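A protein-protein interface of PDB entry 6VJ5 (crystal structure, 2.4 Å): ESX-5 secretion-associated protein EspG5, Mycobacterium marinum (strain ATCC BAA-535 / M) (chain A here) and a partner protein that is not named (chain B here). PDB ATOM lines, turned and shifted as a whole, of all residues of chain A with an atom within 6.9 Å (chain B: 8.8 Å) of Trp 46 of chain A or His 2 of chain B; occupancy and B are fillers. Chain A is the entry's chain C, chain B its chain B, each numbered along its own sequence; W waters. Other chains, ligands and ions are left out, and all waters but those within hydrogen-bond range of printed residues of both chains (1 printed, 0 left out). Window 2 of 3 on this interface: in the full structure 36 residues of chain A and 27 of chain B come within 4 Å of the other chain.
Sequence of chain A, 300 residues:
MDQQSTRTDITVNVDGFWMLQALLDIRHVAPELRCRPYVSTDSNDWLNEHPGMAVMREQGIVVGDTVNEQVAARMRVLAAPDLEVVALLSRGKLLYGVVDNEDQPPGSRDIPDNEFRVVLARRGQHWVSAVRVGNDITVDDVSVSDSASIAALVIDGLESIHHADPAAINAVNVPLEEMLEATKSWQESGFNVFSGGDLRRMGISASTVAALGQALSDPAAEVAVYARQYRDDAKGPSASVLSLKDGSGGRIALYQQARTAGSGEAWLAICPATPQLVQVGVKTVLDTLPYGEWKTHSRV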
ATOM      1  N   TRP A  18     -21.494   5.090  -9.566  1.00  0.00           N
ATOM      2  CA  TRP A  18     -20.561   6.198  -9.720  1.00  0.00           C
ATOM      3  C   TRP A  18     -19.121   5.757  -9.488  1.00  0.00           C
ATOM      4  O   TRP A  18     -18.210   6.266 -10.147  1.00  0.00           O
ATOM      5  CB  TRP A  18     -20.952   7.324  -8.767  1.00  0.00           C
ATOM      6  CG  TRP A  18     -19.927   8.389  -8.591  1.00  0.00           C
ATOM      7  CD1 TRP A  18     -19.716   9.468  -9.398  1.00  0.00           C
ATOM      8  CD2 TRP A  18     -18.981   8.491  -7.526  1.00  0.00           C
ATOM      9  NE1 TRP A  18     -18.691  10.238  -8.901  1.00  0.00           N
ATOM     10  CE2 TRP A  18     -18.222   9.656  -7.752  1.00  0.00           C
ATOM     11  CE3 TRP A  18     -18.698   7.707  -6.405  1.00  0.00           C
ATOM     12  CZ2 TRP A  18     -17.201  10.055  -6.899  1.00  0.00           C
ATOM     13  CZ3 TRP A  18     -17.690   8.105  -5.560  1.00  0.00           C
ATOM     14  CH2 TRP A  18     -16.954   9.271  -5.808  1.00  0.00           C
ATOM     15  N   MET A  19     -18.893   4.812  -8.577  1.00  0.00           N
ATOM     16  CA  MET A  19     -17.535   4.332  -8.354  1.00  0.00           C
ATOM     17  C   MET A  19     -17.010   3.585  -9.572  1.00  0.00           C
ATOM     18  O   MET A  19     -15.859   3.785  -9.978  1.00  0.00           O
ATOM     19  CB  MET A  19     -17.503   3.452  -7.110  1.00  0.00           C
ATOM     20  CG  MET A  19     -18.204   4.109  -5.931  1.00  0.00           C
ATOM     21  SD  MET A  19     -17.592   3.606  -4.319  1.00  0.00           S
ATOM     22  CE  MET A  19     -17.853   1.838  -4.414  1.00  0.00           C
ATOM     23  N   ARG A  36     -24.339  10.546 -10.288  1.00  0.00           N
ATOM     24  CA  ARG A  36     -23.403  11.619  -9.990  1.00  0.00           C
ATOM     25  C   ARG A  36     -22.361  11.670 -11.101  1.00  0.00           C
ATOM     26  O   ARG A  36     -21.869  10.618 -11.528  1.00  0.00           O
ATOM     27  CB  ARG A  36     -22.730  11.405  -8.638  1.00  0.00           C
ATOM     28  CG  ARG A  36     -22.841  12.613  -7.707  1.00  0.00           C
ATOM     29  CD  ARG A  36     -21.918  12.471  -6.501  1.00  0.00           C
ATOM     30  NE  ARG A  36     -22.089  11.193  -5.816  1.00  0.00           N
ATOM     31  CZ  ARG A  36     -21.201  10.669  -4.975  1.00  0.00           C
ATOM     32  NH1 ARG A  36     -21.440   9.499  -4.399  1.00  0.00           N
ATOM     33  NH2 ARG A  36     -20.069  11.311  -4.713  1.00  0.00           N
ATOM     34  N   TYR A  38     -18.686  12.003 -12.609  1.00  0.00           N
ATOM     35  CA  TYR A  38     -17.357  11.709 -12.092  1.00  0.00           C
ATOM     36  C   TYR A  38     -16.375  12.722 -12.662  1.00  0.00           C
ATOM     37  O   TYR A  38     -16.392  12.999 -13.864  1.00  0.00           O
ATOM     38  CB  TYR A  38     -16.898  10.294 -12.442  1.00  0.00           C
ATOM     39  CG  TYR A  38     -15.412  10.096 -12.218  1.00  0.00           C
ATOM     40  CD1 TYR A  38     -14.875  10.100 -10.938  1.00  0.00           C
ATOM     41  CD2 TYR A  38     -14.544   9.924 -13.290  1.00  0.00           C
ATOM     42  CE1 TYR A  38     -13.518   9.931 -10.730  1.00  0.00           C
ATOM     43  CE2 TYR A  38     -13.186   9.752 -13.090  1.00  0.00           C
ATOM     44  CZ  TYR A  38     -12.681   9.758 -11.809  1.00  0.00           C
ATOM     45  OH  TYR A  38     -11.334   9.585 -11.604  1.00  0.00           O
ATOM     46  N   VAL A  39     -15.519  13.265 -11.800  1.00  0.00           N
ATOM     47  CA  VAL A  39     -14.543  14.279 -12.183  1.00  0.00           C
ATOM     48  C   VAL A  39     -13.161  13.764 -11.813  1.00  0.00           C
ATOM     49  O   VAL A  39     -12.877  13.517 -10.632  1.00  0.00           O
ATOM     50  CB  VAL A  39     -14.832  15.628 -11.507  1.00  0.00           C
ATOM     51  CG1 VAL A  39     -13.697  16.604 -11.756  1.00  0.00           C
ATOM     52  CG2 VAL A  39     -16.156  16.188 -12.015  1.00  0.00           C
ATOM     53  N   THR A  41      -9.441  13.540 -10.762  1.00  0.00           N
ATOM     54  CA  THR A  41      -8.667  14.330  -9.816  1.00  0.00           C
ATOM     55  C   THR A  41      -7.279  13.704  -9.723  1.00  0.00           C
ATOM     56  O   THR A  41      -6.862  12.935 -10.597  1.00  0.00           O
ATOM     57  CB  THR A  41      -9.377  14.402  -8.454  1.00  0.00           C
ATOM     58  OG1 THR A  41      -9.639  13.075  -7.975  1.00  0.00           O
ATOM     59  CG2 THR A  41     -10.688  15.168  -8.568  1.00  0.00           C
ATOM     60  N   SER A  43      -6.466  11.685  -7.213  1.00  0.00           N
ATOM     61  CA  SER A  43      -6.550  10.417  -6.503  1.00  0.00           C
ATOM     62  C   SER A  43      -7.979   9.895  -6.501  1.00  0.00           C
ATOM     63  O   SER A  43      -8.927  10.654  -6.291  1.00  0.00           O
ATOM     64  CB  SER A  43      -6.049  10.564  -5.059  1.00  0.00           C
ATOM     65  OG  SER A  43      -5.846   9.297  -4.458  1.00  0.00           O
ATOM     66  N   ASN A  44      -8.115   8.590  -6.735  1.00  0.00           N
ATOM     67  CA  ASN A  44      -9.370   7.875  -6.561  1.00  0.00           C
ATOM     68  C   ASN A  44      -9.316   6.897  -5.393  1.00  0.00           C
ATOM     69  O   ASN A  44     -10.192   6.032  -5.283  1.00  0.00           O
ATOM     70  CB  ASN A  44      -9.738   7.134  -7.850  1.00  0.00           C
ATOM     71  CG  ASN A  44     -10.572   7.985  -8.804  1.00  0.00           C
ATOM     72  OD1 ASN A  44     -10.904   9.135  -8.509  1.00  0.00           O
ATOM     73  ND2 ASN A  44     -10.913   7.419  -9.955  1.00  0.00           N
ATOM     74  N   ASP A  45      -8.312   7.013  -4.517  1.00  0.00           N
ATOM     75  CA  ASP A  45      -8.173   6.098  -3.388  1.00  0.00           C
ATOM     76  C   ASP A  45      -9.189   6.375  -2.282  1.00  0.00           C
ATOM     77  O   ASP A  45      -9.494   5.471  -1.496  1.00  0.00           O
ATOM     78  CB  ASP A  45      -6.749   6.174  -2.823  1.00  0.00           C
ATOM     79  CG  ASP A  45      -6.469   5.094  -1.784  1.00  0.00           C
ATOM     80  OD1 ASP A  45      -7.311   4.180  -1.615  1.00  0.00           O
ATOM     81  OD2 ASP A  45      -5.407   5.160  -1.128  1.00  0.00           O
ATOM     82  N   TRP A  46      -9.716   7.601  -2.198  1.00  0.00           N
ATOM     83  CA  TRP A  46     -10.797   7.879  -1.257  1.00  0.00           C
ATOM     84  C   TRP A  46     -12.066   7.114  -1.613  1.00  0.00           C
ATOM     85  O   TRP A  46     -12.967   7.000  -0.774  1.00  0.00           O
ATOM     86  CB  TRP A  46     -11.086   9.382  -1.196  1.00  0.00           C
ATOM     87  CG  TRP A  46     -11.748   9.957  -2.420  1.00  0.00           C
ATOM     88  CD1 TRP A  46     -11.154  10.244  -3.620  1.00  0.00           C
ATOM     89  CD2 TRP A  46     -13.125  10.340  -2.553  1.00  0.00           C
ATOM     90  NE1 TRP A  46     -12.081  10.771  -4.492  1.00  0.00           N
ATOM     91  CE2 TRP A  46     -13.296  10.841  -3.861  1.00  0.00           C
ATOM     92  CE3 TRP A  46     -14.230  10.306  -1.693  1.00  0.00           C
ATOM     93  CZ2 TRP A  46     -14.529  11.300  -4.331  1.00  0.00           C
ATOM     94  CZ3 TRP A  46     -15.453  10.762  -2.162  1.00  0.00           C
ATOM     95  CH2 TRP A  46     -15.592  11.253  -3.468  1.00  0.00           C
ATOM     96  N   LEU A  47     -12.151   6.587  -2.838  1.00  0.00           N
ATOM     97  CA  LEU A  47     -13.252   5.700  -3.193  1.00  0.00           C
ATOM     98  C   LEU A  47     -13.200   4.403  -2.393  1.00  0.00           C
ATOM     99  O   LEU A  47     -14.250   3.839  -2.059  1.00  0.00           O
ATOM    100  CB  LEU A  47     -13.212   5.396  -4.692  1.00  0.00           C
ATOM    101  CG  LEU A  47     -13.263   6.609  -5.619  1.00  0.00           C
ATOM    102  CD1 LEU A  47     -13.038   6.218  -7.069  1.00  0.00           C
ATOM    103  CD2 LEU A  47     -14.600   7.311  -5.461  1.00  0.00           C
ATOM    104  N   ASN A  48     -11.991   3.914  -2.081  1.00  0.00           N
ATOM    105  CA  ASN A  48     -11.842   2.678  -1.316  1.00  0.00           C
ATOM    106  C   ASN A  48     -12.477   2.766   0.068  1.00  0.00           C
ATOM    107  O   ASN A  48     -12.685   1.730   0.713  1.00  0.00           O
ATOM    108  CB  ASN A  48     -10.359   2.325  -1.163  1.00  0.00           C
ATOM    109  CG  ASN A  48      -9.860   1.389  -2.247  1.00  0.00           C
ATOM    110  OD1 ASN A  48     -10.606   0.549  -2.747  1.00  0.00           O
ATOM    111  ND2 ASN A  48      -8.588   1.524  -2.607  1.00  0.00           N
ATOM    112  N   GLU A  49     -12.766   3.977   0.549  1.00  0.00           N
ATOM    113  CA  GLU A  49     -13.406   4.157   1.844  1.00  0.00           C
ATOM    114  C   GLU A  49     -14.919   3.986   1.783  1.00  0.00           C
ATOM    115  O   GLU A  49     -15.536   3.694   2.812  1.00  0.00           O
ATOM    116  CB  GLU A  49     -13.055   5.543   2.401  1.00  0.00           C
ATOM    117  CG  GLU A  49     -11.682   5.611   3.069  1.00  0.00           C
ATOM    118  CD  GLU A  49     -11.066   7.003   3.055  1.00  0.00           C
ATOM    119  OE1 GLU A  49     -11.762   7.980   2.699  1.00  0.00           O
ATOM    120  OE2 GLU A  49      -9.868   7.115   3.397  1.00  0.00           O
ATOM    121  N   HIS A  50     -15.528   4.153   0.615  1.00  0.00           N
ATOM    122  CA  HIS A  50     -16.970   4.003   0.512  1.00  0.00           C
ATOM    123  C   HIS A  50     -17.367   2.575   0.884  1.00  0.00           C
ATOM    124  O   HIS A  50     -16.670   1.621   0.514  1.00  0.00           O
ATOM    125  CB  HIS A  50     -17.441   4.330  -0.906  1.00  0.00           C
ATOM    126  CG  HIS A  50     -18.852   4.826  -0.974  1.00  0.00           C
ATOM    127  ND1 HIS A  50     -19.942   3.988  -0.887  1.00  0.00           N
ATOM    128  CD2 HIS A  50     -19.349   6.077  -1.120  1.00  0.00           C
ATOM    129  CE1 HIS A  50     -21.051   4.701  -0.972  1.00  0.00           C
ATOM    130  NE2 HIS A  50     -20.719   5.970  -1.116  1.00  0.00           N
ATOM    131  N   MET B   1     -10.937  16.943   0.072  1.00  0.00           N
ATOM    132  CA  MET B   1     -12.103  17.831  -0.213  1.00  0.00           C
ATOM    133  C   MET B   1     -12.621  17.497  -1.620  1.00  0.00           C
ATOM    134  O   MET B   1     -11.980  17.839  -2.617  1.00  0.00           O
ATOM    135  CB  MET B   1     -11.723  19.309  -0.129  1.00  0.00           C
ATOM    136  CG  MET B   1     -10.654  19.673   0.898  1.00  0.00           C
ATOM    137  SD  MET B   1     -10.039  21.362   0.668  1.00  0.00           S
ATOM    138  CE  MET B   1      -8.334  21.194   1.202  1.00  0.00           C
ATOM    139  N   HIS B   2     -13.770  16.839  -1.713  1.00  0.00           N
ATOM    140  CA  HIS B   2     -14.247  16.281  -2.976  1.00  0.00           C
ATOM    141  C   HIS B   2     -15.475  17.054  -3.444  1.00  0.00           C
ATOM    142  O   HIS B   2     -16.600  16.549  -3.458  1.00  0.00           O
ATOM    143  CB  HIS B   2     -14.538  14.799  -2.792  1.00  0.00           C
ATOM    144  CG  HIS B   2     -13.447  14.062  -2.080  1.00  0.00           C
ATOM    145  ND1 HIS B   2     -12.182  13.918  -2.606  1.00  0.00           N
ATOM    146  CD2 HIS B   2     -13.430  13.435  -0.881  1.00  0.00           C
ATOM    147  CE1 HIS B   2     -11.433  13.232  -1.763  1.00  0.00           C
ATOM    148  NE2 HIS B   2     -12.168  12.924  -0.709  1.00  0.00           N
ATOM    149  N   PHE B   3     -15.239  18.305  -3.844  1.00  0.00           N
ATOM    150  CA  PHE B   3     -16.344  19.200  -4.165  1.00  0.00           C
ATOM    151  C   PHE B   3     -17.149  18.733  -5.362  1.00  0.00           C
ATOM    152  O   PHE B   3     -18.288  19.181  -5.537  1.00  0.00           O
ATOM    153  CB  PHE B   3     -15.805  20.600  -4.410  1.00  0.00           C
ATOM    154  CG  PHE B   3     -14.926  21.090  -3.308  1.00  0.00           C
ATOM    155  CD1 PHE B   3     -15.470  21.689  -2.190  1.00  0.00           C
ATOM    156  CD2 PHE B   3     -13.554  20.933  -3.378  1.00  0.00           C
ATOM    157  CE1 PHE B   3     -14.666  22.130  -1.171  1.00  0.00           C
ATOM    158  CE2 PHE B   3     -12.747  21.375  -2.359  1.00  0.00           C
ATOM    159  CZ  PHE B   3     -13.304  21.974  -1.255  1.00  0.00           C
ATOM    160  N   GLU B   4     -16.593  17.838  -6.182  1.00  0.00           N
ATOM    161  CA  GLU B   4     -17.344  17.275  -7.299  1.00  0.00           C
ATOM    162  C   GLU B   4     -18.575  16.500  -6.841  1.00  0.00           C
ATOM    163  O   GLU B   4     -19.405  16.137  -7.682  1.00  0.00           O
ATOM    164  CB  GLU B   4     -16.433  16.370  -8.150  1.00  0.00           C
ATOM    165  CG  GLU B   4     -15.908  15.102  -7.469  1.00  0.00           C
ATOM    166  CD  GLU B   4     -14.567  15.305  -6.771  1.00  0.00           C
ATOM    167  OE1 GLU B   4     -14.253  16.461  -6.414  1.00  0.00           O
ATOM    168  OE2 GLU B   4     -13.827  14.310  -6.583  1.00  0.00           O
ATOM    169  N   ALA B   5     -18.710  16.236  -5.542  1.00  0.00           N
ATOM    170  CA  ALA B   5     -19.883  15.577  -4.980  1.00  0.00           C
ATOM    171  C   ALA B   5     -20.993  16.551  -4.617  1.00  0.00           C
ATOM    172  O   ALA B   5     -22.047  16.121  -4.144  1.00  0.00           O
ATOM    173  CB  ALA B   5     -19.499  14.784  -3.725  1.00  0.00           C
ATOM    174  N   TYR B   6     -20.782  17.820  -4.788  1.00  0.00           N
ATOM    175  CA  TYR B   6     -21.795  18.796  -4.459  1.00  0.00           C
ATOM    176  C   TYR B   6     -22.341  19.415  -5.736  1.00  0.00           C
ATOM    177  O   TYR B   6     -21.612  19.590  -6.717  1.00  0.00           O
ATOM    178  CB  TYR B   6     -21.234  19.899  -3.561  1.00  0.00           C
ATOM    179  CG  TYR B   6     -20.600  19.401  -2.277  1.00  0.00           C
ATOM    180  CD1 TYR B   6     -21.183  18.390  -1.518  1.00  0.00           C
ATOM    181  CD2 TYR B   6     -19.419  19.956  -1.824  1.00  0.00           C
ATOM    182  CE1 TYR B   6     -20.597  17.958  -0.349  1.00  0.00           C
ATOM    183  CE2 TYR B   6     -18.830  19.530  -0.661  1.00  0.00           C
ATOM    184  CZ  TYR B   6     -19.419  18.536   0.074  1.00  0.00           C
ATOM    185  OH  TYR B   6     -18.805  18.130   1.229  1.00  0.00           O
ATOM    186  N   PRO B   7     -23.627  19.744  -5.764  1.00  0.00           N
ATOM    187  CA  PRO B   7     -24.242  20.230  -7.003  1.00  0.00           C
ATOM    188  C   PRO B   7     -23.797  21.645  -7.318  1.00  0.00           C
ATOM    189  O   PRO B   7     -23.297  22.357  -6.435  1.00  0.00           O
ATOM    190  CB  PRO B   7     -25.744  20.164  -6.699  1.00  0.00           C
ATOM    191  CG  PRO B   7     -25.825  20.359  -5.213  1.00  0.00           C
ATOM    192  CD  PRO B   7     -24.583  19.701  -4.639  1.00  0.00           C
ATOM    193  N   ASN B  11     -21.387  24.909  -5.157  1.00  0.00           N
ATOM    194  CA  ASN B  11     -20.050  25.393  -5.484  1.00  0.00           C
ATOM    195  C   ASN B  11     -20.099  26.808  -6.049  1.00  0.00           C
ATOM    196  O   ASN B  11     -19.279  27.664  -5.680  1.00  0.00           O
ATOM    197  CB  ASN B  11     -19.379  24.419  -6.452  1.00  0.00           C
ATOM    198  CG  ASN B  11     -18.980  23.129  -5.776  1.00  0.00           C
ATOM    199  OD1 ASN B  11     -18.502  23.141  -4.647  1.00  0.00           O
ATOM    200  ND2 ASN B  11     -19.192  22.008  -6.453  1.00  0.00           N
ATOM    201  N   TRP B 143     -22.397  20.917 -13.227  1.00  0.00           N
ATOM    202  CA  TRP B 143     -21.890  20.180 -12.071  1.00  0.00           C
ATOM    203  C   TRP B 143     -20.437  19.781 -12.268  1.00  0.00           C
ATOM    204  O   TRP B 143     -19.602  19.949 -11.373  1.00  0.00           O
ATOM    205  CB  TRP B 143     -22.771  18.943 -11.858  1.00  0.00           C
ATOM    206  CG  TRP B 143     -22.576  18.173 -10.599  1.00  0.00           C
ATOM    207  CD1 TRP B 143     -21.405  17.895  -9.978  1.00  0.00           C
ATOM    208  CD2 TRP B 143     -23.604  17.570  -9.809  1.00  0.00           C
ATOM    209  NE1 TRP B 143     -21.631  17.148  -8.850  1.00  0.00           N
ATOM    210  CE2 TRP B 143     -22.977  16.940  -8.720  1.00  0.00           C
ATOM    211  CE3 TRP B 143     -24.994  17.502  -9.918  1.00  0.00           C
ATOM    212  CZ2 TRP B 143     -23.691  16.257  -7.743  1.00  0.00           C
ATOM    213  CZ3 TRP B 143     -25.702  16.824  -8.949  1.00  0.00           C
ATOM    214  CH2 TRP B 143     -25.051  16.209  -7.876  1.00  0.00           C
ATOM    215  N   ASP B 146     -17.995  23.020 -12.310  1.00  0.00           N
ATOM    216  CA  ASP B 146     -17.723  23.526 -10.969  1.00  0.00           C
ATOM    217  C   ASP B 146     -16.817  22.577 -10.196  1.00  0.00           C
ATOM    218  O   ASP B 146     -15.954  23.014  -9.427  1.00  0.00           O
ATOM    219  CB  ASP B 146     -19.028  23.738 -10.201  1.00  0.00           C
ATOM    220  CG  ASP B 146     -19.655  25.086 -10.472  1.00  0.00           C
ATOM    221  OD1 ASP B 146     -19.251  25.755 -11.448  1.00  0.00           O
ATOM    222  OD2 ASP B 146     -20.550  25.479  -9.695  1.00  0.00           O
ATOM    223  N   GLY B 147     -17.014  21.272 -10.366  1.00  0.00           N
ATOM    224  CA  GLY B 147     -16.141  20.322  -9.707  1.00  0.00           C
ATOM    225  C   GLY B 147     -14.704  20.453 -10.165  1.00  0.00           C
ATOM    226  O   GLY B 147     -13.775  20.336  -9.363  1.00  0.00           O
ATOM    227  N   MET B 150     -13.154  23.792  -8.645  1.00  0.00           N
ATOM    228  CA  MET B 150     -12.782  23.660  -7.241  1.00  0.00           C
ATOM    229  C   MET B 150     -11.583  22.728  -7.079  1.00  0.00           C
ATOM    230  O   MET B 150     -10.711  22.967  -6.232  1.00  0.00           O
ATOM    231  CB  MET B 150     -13.975  23.161  -6.430  1.00  0.00           C
ATOM    232  CG  MET B 150     -15.050  24.213  -6.234  1.00  0.00           C
ATOM    233  SD  MET B 150     -14.461  25.669  -5.324  1.00  0.00           S
ATOM    234  CE  MET B 150     -13.999  24.915  -3.769  1.00  0.00           C
ATOM    235  N   ARG B 151     -11.523  21.652  -7.874  1.00  0.00           N
ATOM    236  CA  ARG B 151     -10.325  20.814  -7.890  1.00  0.00           C
ATOM    237  C   ARG B 151      -9.075  21.665  -8.111  1.00  0.00           C
ATOM    238  O   ARG B 151      -8.125  21.614  -7.321  1.00  0.00           O
ATOM    239  CB  ARG B 151     -10.440  19.731  -8.976  1.00  0.00           C
ATOM    240  CG  ARG B 151      -9.234  18.794  -9.107  1.00  0.00           C
ATOM    241  CD  ARG B 151      -9.245  18.058 -10.467  1.00  0.00           C
ATOM    242  NE  ARG B 151      -9.275  19.005 -11.588  1.00  0.00           N
ATOM    243  CZ  ARG B 151      -9.718  18.727 -12.812  1.00  0.00           C
ATOM    244  NH1 ARG B 151     -10.180  17.521 -13.103  1.00  0.00           N
ATOM    245  NH2 ARG B 151      -9.708  19.668 -13.745  1.00  0.00           N
ATOM    246  N   ARG B 154      -8.326  24.102  -5.163  1.00  0.00           N
ATOM    247  CA  ARG B 154      -7.719  23.406  -4.036  1.00  0.00           C
ATOM    248  C   ARG B 154      -6.253  23.100  -4.301  1.00  0.00           C
ATOM    249  O   ARG B 154      -5.413  23.248  -3.409  1.00  0.00           O
ATOM    250  CB  ARG B 154      -8.489  22.120  -3.747  1.00  0.00           C
ATOM    251  CG  ARG B 154      -7.781  21.214  -2.764  1.00  0.00           C
ATOM    252  CD  ARG B 154      -8.552  19.938  -2.501  1.00  0.00           C
ATOM    253  NE  ARG B 154      -8.707  19.083  -3.679  1.00  0.00           N
ATOM    254  CZ  ARG B 154      -7.791  18.219  -4.115  1.00  0.00           C
ATOM    255  NH1 ARG B 154      -6.624  18.100  -3.495  1.00  0.00           N
ATOM    256  NH2 ARG B 154      -8.046  17.476  -5.182  1.00  0.00           N
HETATM  257  O   HOH W   1     -13.750  12.422  -8.389  1.00  0.00           O
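Water W1 lies within hydrogen-bond range of the side-chain carboxylate of Glu 4 of chain B (2.6 Å) and the backbone carbonyl oxygen of Val 39 of chain A (2.6 Å).
Printed residues of chain B within 4 Å of Thr 41 of chain A: Glu 4 (3.8 Å) and Arg 151 (3.7 Å). Asp 45 of chain A touches none of the printed residues of chain B. Of chain B, only His 2 and Glu 4 come within 4 Å of Trp 46 of chain A. Asn 48 of chain A touches none of the printed residues of chain B. His 2 of chain B touches just one residue of chain A: Trp 46 (3.3 Å). Of the printed residues of chain A, Glu 4 of chain B touches Val 39, Thr 41 and Trp 46. Of the printed residues of chain A, Trp 143 of chain B touches Arg 36. Printed residues of chain A within 4 Å of Arg 151 of chain B: Val 39 and Thr 41. The nearest printed residue of chain B that does not touch Val 39 of chain A is Gly 147 of chain B (4.3 Å).
Arg 36 of chain A touches Ala 5 of chain B (NH2 to CB, 3.7 Å). Arg 36 of chain A touches Trp 143 of chain B (CG to CZ2, 3.7 Å). CB of Glu 4 of chain B touches CB of Val 39 of chain A, 3.8 Å away. NH1 of Arg 151 of chain B touches CG1 of Val 39 of chain A, at 3.9 Å. CG2 of Thr 41 of chain A touches OE2 of Glu 4 of chain B, at 3.8 Å. Arg 151 of chain B touches Thr 41 of chain A. CD2 of Trp 46 of chain A touches NE2 of His 2 of chain B, 3.3 Å away. Glu 4 of chain B touches Trp 46 of chain A (OE2 to CZ2, 3.8 Å).
NE1 of Trp 143 of chain B is in hydrogen-bond range of O of Glu 4 of chain B (2.7 Å). NE1 of Trp 143 of chain B lies within hydrogen-bond range of O of Tyr 6 of chain B (3.2 Å). OG1 of Thr 41 of chain A lies within hydrogen-bond range of O of Ser 43 of chain A, 3.0 Å away.
Printed residues of chain B that touch a printed residue of chain A: His 2, Glu 4, Ala 5, Trp 143 and Arg 151. Along chain B the printed residues that touch a printed residue of chain A span positions 2 to 151. Of the 14 printed residues of chain A, 4 touch a printed residue of chain B. Hydrophobic or aromatic side chains of chain A within 4 Å of the printed part of chain B: Val 39 and Trp 46. Among the printed residues, no Asp or Glu carboxylate lies within 4 Å of a Lys or Arg side-chain nitrogen of the other chain.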
